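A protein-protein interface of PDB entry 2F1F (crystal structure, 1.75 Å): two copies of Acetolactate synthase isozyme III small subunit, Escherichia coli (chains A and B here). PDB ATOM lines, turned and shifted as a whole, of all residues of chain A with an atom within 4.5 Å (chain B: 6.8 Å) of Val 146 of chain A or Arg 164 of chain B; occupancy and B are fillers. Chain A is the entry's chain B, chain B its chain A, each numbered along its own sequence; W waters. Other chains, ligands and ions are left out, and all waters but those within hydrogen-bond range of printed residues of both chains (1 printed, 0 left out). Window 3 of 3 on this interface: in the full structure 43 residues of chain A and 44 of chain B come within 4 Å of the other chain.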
ATOM      1  N   LYS A  91       7.982  22.759 -25.683  1.00  0.00           N
ATOM      2  CA  LYS A  91       7.642  22.186 -26.993  1.00  0.00           C
ATOM      3  C   LYS A  91       7.569  23.346 -27.958  1.00  0.00           C
ATOM      4  O   LYS A  91       6.821  24.336 -27.717  1.00  0.00           O
ATOM      5  CB  LYS A  91       6.371  21.361 -26.960  1.00  0.00           C
ATOM      6  CG  LYS A  91       6.045  20.603 -28.248  1.00  0.00           C
ATOM      7  CD  LYS A  91       4.797  19.732 -28.117  1.00  0.00           C
ATOM      8  CE  LYS A  91       4.914  18.493 -27.283  1.00  0.00           C
ATOM      9  NZ  LYS A  91       3.500  17.986 -27.034  1.00  0.00           N
ATOM     10  N   ILE A  92       8.290  23.232 -29.079  1.00  0.00           N
ATOM     11  CA  ILE A  92       8.490  24.343 -30.027  1.00  0.00           C
ATOM     12  C   ILE A  92       8.234  23.885 -31.467  1.00  0.00           C
ATOM     13  O   ILE A  92       8.745  22.843 -31.915  1.00  0.00           O
ATOM     14  CB  ILE A  92       9.887  24.954 -29.914  1.00  0.00           C
ATOM     15  CG1 ILE A  92      10.230  25.315 -28.491  1.00  0.00           C
ATOM     16  CG2 ILE A  92      10.010  26.227 -30.851  1.00  0.00           C
ATOM     17  CD1 ILE A  92      11.762  25.535 -28.218  1.00  0.00           C
ATOM     18  N   GLN A  93       7.460  24.693 -32.183  1.00  0.00           N
ATOM     19  CA  GLN A  93       7.248  24.520 -33.607  1.00  0.00           C
ATOM     20  C   GLN A  93       8.565  24.813 -34.283  1.00  0.00           C
ATOM     21  O   GLN A  93       9.149  25.910 -34.123  1.00  0.00           O
ATOM     22  CB  GLN A  93       6.222  25.562 -34.113  1.00  0.00           C
ATOM     23  CG  GLN A  93       4.894  25.234 -33.628  1.00  0.00           C
ATOM     24  CD  GLN A  93       4.255  24.104 -34.399  1.00  0.00           C
ATOM     25  OE1 GLN A  93       4.863  23.549 -35.315  1.00  0.00           O
ATOM     26  NE2 GLN A  93       3.000  23.761 -34.036  1.00  0.00           N
ATOM     27  N   LYS A 144       7.612  29.318 -32.802  1.00  0.00           N
ATOM     28  CA  LYS A 144       6.409  29.332 -31.937  1.00  0.00           C
ATOM     29  C   LYS A 144       6.517  28.363 -30.767  1.00  0.00           C
ATOM     30  O   LYS A 144       6.556  27.131 -30.949  1.00  0.00           O
ATOM     31  CB  LYS A 144       5.154  29.001 -32.737  1.00  0.00           C
ATOM     32  CG  LYS A 144       3.871  28.795 -31.911  1.00  0.00           C
ATOM     33  CD  LYS A 144       3.394  30.043 -31.291  1.00  0.00           C
ATOM     34  CE  LYS A 144       1.961  29.941 -30.741  1.00  0.00           C
ATOM     35  NZ  LYS A 144       0.898  30.301 -31.730  1.00  0.00           N
ATOM     36  N   ILE A 145       6.542  28.910 -29.569  1.00  0.00           N
ATOM     37  CA  ILE A 145       6.473  28.075 -28.341  1.00  0.00           C
ATOM     38  C   ILE A 145       5.075  27.580 -28.190  1.00  0.00           C
ATOM     39  O   ILE A 145       4.138  28.419 -28.035  1.00  0.00           O
ATOM     40  CB  ILE A 145       6.966  28.828 -27.113  1.00  0.00           C
ATOM     41  CG1 ILE A 145       8.478  29.221 -27.316  1.00  0.00           C
ATOM     42  CG2 ILE A 145       6.665  28.016 -25.792  1.00  0.00           C
ATOM     43  CD1 ILE A 145       8.952  30.307 -26.291  1.00  0.00           C
ATOM     44  N   VAL A 146       4.883  26.269 -28.203  1.00  0.00           N
ATOM     45  CA  VAL A 146       3.497  25.714 -28.121  1.00  0.00           C
ATOM     46  C   VAL A 146       3.067  25.262 -26.725  1.00  0.00           C
ATOM     47  O   VAL A 146       1.890  25.380 -26.365  1.00  0.00           O
ATOM     48  CB  VAL A 146       3.128  24.636 -29.160  1.00  0.00           C
ATOM     49  CG1 VAL A 146       3.336  25.123 -30.634  1.00  0.00           C
ATOM     50  CG2 VAL A 146       3.786  23.405 -28.964  1.00  0.00           C
ATOM     51  N   GLU A 147       4.000  24.769 -25.923  1.00  0.00           N
ATOM     52  CA  GLU A 147       3.751  24.313 -24.576  1.00  0.00           C
ATOM     53  C   GLU A 147       5.016  24.534 -23.739  1.00  0.00           C
ATOM     54  O   GLU A 147       6.149  24.406 -24.244  1.00  0.00           O
ATOM     55  CB  GLU A 147       3.396  22.802 -24.498  1.00  0.00           C
ATOM     56  CG  GLU A 147       2.173  22.353 -25.163  1.00  0.00           C
ATOM     57  CD  GLU A 147       1.843  20.874 -24.857  1.00  0.00           C
ATOM     58  OE1 GLU A 147       2.541  19.967 -25.356  1.00  0.00           O
ATOM     59  OE2 GLU A 147       0.857  20.640 -24.193  1.00  0.00           O
ATOM     60  N   LEU B   9      -3.770  23.599 -17.162  1.00  0.00           N
ATOM     61  CA  LEU B   9      -3.466  24.961 -17.616  1.00  0.00           C
ATOM     62  C   LEU B   9      -4.382  25.909 -16.799  1.00  0.00           C
ATOM     63  O   LEU B   9      -5.601  25.754 -16.835  1.00  0.00           O
ATOM     64  CB  LEU B   9      -3.764  25.138 -19.097  1.00  0.00           C
ATOM     65  CG  LEU B   9      -3.199  26.387 -19.766  1.00  0.00           C
ATOM     66  CD1 LEU B   9      -1.641  26.612 -19.560  1.00  0.00           C
ATOM     67  CD2 LEU B   9      -3.533  26.372 -21.243  1.00  0.00           C
ATOM     68  N   ARG B  46       1.186  26.487 -15.856  1.00  0.00           N
ATOM     69  CA  ARG B  46       0.963  25.036 -16.082  1.00  0.00           C
ATOM     70  C   ARG B  46       1.346  24.282 -14.811  1.00  0.00           C
ATOM     71  O   ARG B  46       2.397  24.548 -14.203  1.00  0.00           O
ATOM     72  CB  ARG B  46       1.829  24.522 -17.242  1.00  0.00           C
ATOM     73  CG  ARG B  46       1.524  23.083 -17.540  1.00  0.00           C
ATOM     74  CD  ARG B  46       1.706  22.736 -18.944  1.00  0.00           C
ATOM     75  NE  ARG B  46       1.409  21.326 -19.210  1.00  0.00           N
ATOM     76  CZ  ARG B  46       1.152  20.829 -20.429  1.00  0.00           C
ATOM     77  NH1 ARG B  46       1.176  21.630 -21.479  1.00  0.00           N
ATOM     78  NH2 ARG B  46       0.907  19.538 -20.600  1.00  0.00           N
ATOM     79  N   ARG B  73      -7.716  24.021 -19.065  1.00  0.00           N
ATOM     80  CA  ARG B  73      -7.597  22.708 -19.667  1.00  0.00           C
ATOM     81  C   ARG B  73      -7.040  21.761 -18.591  1.00  0.00           C
ATOM     82  O   ARG B  73      -6.294  22.186 -17.683  1.00  0.00           O
ATOM     83  CB  ARG B  73      -6.553  22.754 -20.787  1.00  0.00           C
ATOM     84  CG  ARG B  73      -7.010  22.654 -22.142  1.00  0.00           C
ATOM     85  CD  ARG B  73      -7.496  23.953 -22.537  1.00  0.00           C
ATOM     86  NE  ARG B  73      -8.018  23.997 -23.897  1.00  0.00           N
ATOM     87  CZ  ARG B  73      -9.033  24.768 -24.253  1.00  0.00           C
ATOM     88  NH1 ARG B  73      -9.649  25.528 -23.337  1.00  0.00           N
ATOM     89  NH2 ARG B  73      -9.450  24.767 -25.511  1.00  0.00           N
ATOM     90  N   GLY B 159       5.061  14.594 -28.936  1.00  0.00           N
ATOM     91  CA  GLY B 159       4.623  14.742 -30.303  1.00  0.00           C
ATOM     92  C   GLY B 159       3.543  15.760 -30.477  1.00  0.00           C
ATOM     93  O   GLY B 159       3.496  16.753 -29.744  1.00  0.00           O
ATOM     94  N   ASP B 160       2.644  15.546 -31.434  1.00  0.00           N
ATOM     95  CA  ASP B 160       1.679  16.614 -31.698  1.00  0.00           C
ATOM     96  C   ASP B 160       0.429  16.605 -30.801  1.00  0.00           C
ATOM     97  O   ASP B 160      -0.543  17.329 -31.069  1.00  0.00           O
ATOM     98  CB  ASP B 160       1.309  16.717 -33.188  1.00  0.00           C
ATOM     99  CG  ASP B 160       0.476  15.585 -33.663  1.00  0.00           C
ATOM    100  OD1 ASP B 160       0.407  14.545 -32.955  1.00  0.00           O
ATOM    101  OD2 ASP B 160      -0.128  15.770 -34.770  1.00  0.00           O
ATOM    102  N   ILE B 162      -0.977  18.182 -27.865  1.00  0.00           N
ATOM    103  CA  ILE B 162      -0.667  19.482 -27.287  1.00  0.00           C
ATOM    104  C   ILE B 162      -1.868  19.969 -26.528  1.00  0.00           C
ATOM    105  O   ILE B 162      -3.005  20.005 -27.105  1.00  0.00           O
ATOM    106  CB  ILE B 162      -0.304  20.498 -28.400  1.00  0.00           C
ATOM    107  CG1 ILE B 162       1.051  20.129 -29.043  1.00  0.00           C
ATOM    108  CG2 ILE B 162      -0.218  21.916 -27.898  1.00  0.00           C
ATOM    109  CD1 ILE B 162       1.275  20.790 -30.442  1.00  0.00           C
ATOM    110  N   MET B 163      -1.661  20.360 -25.268  1.00  0.00           N
ATOM    111  CA  MET B 163      -2.737  20.967 -24.438  1.00  0.00           C
ATOM    112  C   MET B 163      -2.656  22.459 -24.686  1.00  0.00           C
ATOM    113  O   MET B 163      -1.724  23.106 -24.227  1.00  0.00           O
ATOM    114  CB  MET B 163      -2.539  20.677 -22.936  1.00  0.00           C
ATOM    115  CG  MET B 163      -3.746  20.983 -22.008  1.00  0.00           C
ATOM    116  SD  MET B 163      -3.486  20.610 -20.226  1.00  0.00           S
ATOM    117  CE  MET B 163      -2.061  21.552 -19.909  1.00  0.00           C
ATOM    118  N   ARG B 164      -3.592  22.994 -25.463  1.00  0.00           N
ATOM    119  CA  ARG B 164      -3.586  24.462 -25.733  1.00  0.00           C
ATOM    120  C   ARG B 164      -4.994  25.026 -25.531  1.00  0.00           C
ATOM    121  O   ARG B 164      -5.956  24.518 -26.138  1.00  0.00           O
ATOM    122  CB  ARG B 164      -3.072  24.766 -27.157  1.00  0.00           C
ATOM    123  CG  ARG B 164      -3.560  23.733 -28.180  1.00  0.00           C
ATOM    124  CD  ARG B 164      -3.547  24.200 -29.605  1.00  0.00           C
ATOM    125  NE  ARG B 164      -2.237  24.655 -30.063  1.00  0.00           N
ATOM    126  CZ  ARG B 164      -1.504  24.062 -31.018  1.00  0.00           C
ATOM    127  NH1 ARG B 164      -1.908  22.940 -31.599  1.00  0.00           N
ATOM    128  NH2 ARG B 164      -0.344  24.597 -31.395  1.00  0.00           N
HETATM  129  O   HOH W   1       1.102  18.002 -23.059  1.00  0.00           O
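The guanidinium group (NE) of Arg 73 of chain B sits at hydrogen-bond distance from the backbone carbonyl oxygen (O) of Arg 164 of chain B (3.1 Å).
The backbone carbonyl oxygen (O) of Lys 91 of chain A is in hydrogen-bond range of the backbone NH (N) of Val 146 of chain A, at 2.8 Å.
The side-chain amino group (NZ) of Lys 91 of chain A is in salt-bridge range of the side-chain carboxylate (OE1) of Glu 147 of chain A.
CG1 of Ile 162 of chain B touches NZ of Lys 91 of chain A, 3.8 Å away.
Val 146 of chain A touches Ile 162 of chain B.
NH2 of Arg 164 of chain B touches CG1 of Val 146 of chain A, 3.8 Å away.
Glu 147 of chain A touches Ile 162 of chain B (OE2 to CA, 3.6 Å).
OE2 of Glu 147 of chain A sits at hydrogen-bond distance from N of Met 163 of chain B.
NZ of Lys 91 of chain A is in hydrogen-bond range of O of Gly 159 of chain B.
The guanidinium group of Arg 46 of chain B lies within salt-bridge range of the side-chain carboxylate of Glu 147 of chain A.
Of the 8 printed residues of chain B, 5 touch a printed residue of chain A.
Of the 7 printed residues of chain A, 3 touch a printed residue of chain B.
Among the printed residues, 7 pairs touch across the chains.
Among the printed residues, Asp or Glu carboxylates within 4 Å of a Lys or Arg side-chain nitrogen of the other chain: Glu 147 of chain A with Arg 46 of chain B.
Val 146 of chain A touches two residues of chain B.
Of chain A, only Val 146 (3.8 Å) comes within 4 Å of Arg 164 of chain B.
Of the printed residues of chain B, Glu 147 of chain A touches Arg 46 (2.9 Å), Ile 162 (3.6 Å) and Met 163 (2.8 Å).
Of the printed residues of chain A, Gly 159 of chain B touches Lys 91.
Of the printed residues of chain A, Met 163 of chain B touches Glu 147.
Printed residues of chain B within 4 Å of Lys 91 of chain A: Gly 159 (3.0 Å) and Ile 162 (3.8 Å).
Lys 144 of chain A touches none of the printed residues of chain B.
No position is printed for both chains.
Water W1 lies within hydrogen-bond range of OE2 of Glu 147 of chain A and NH2 of Arg 46 of chain B.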
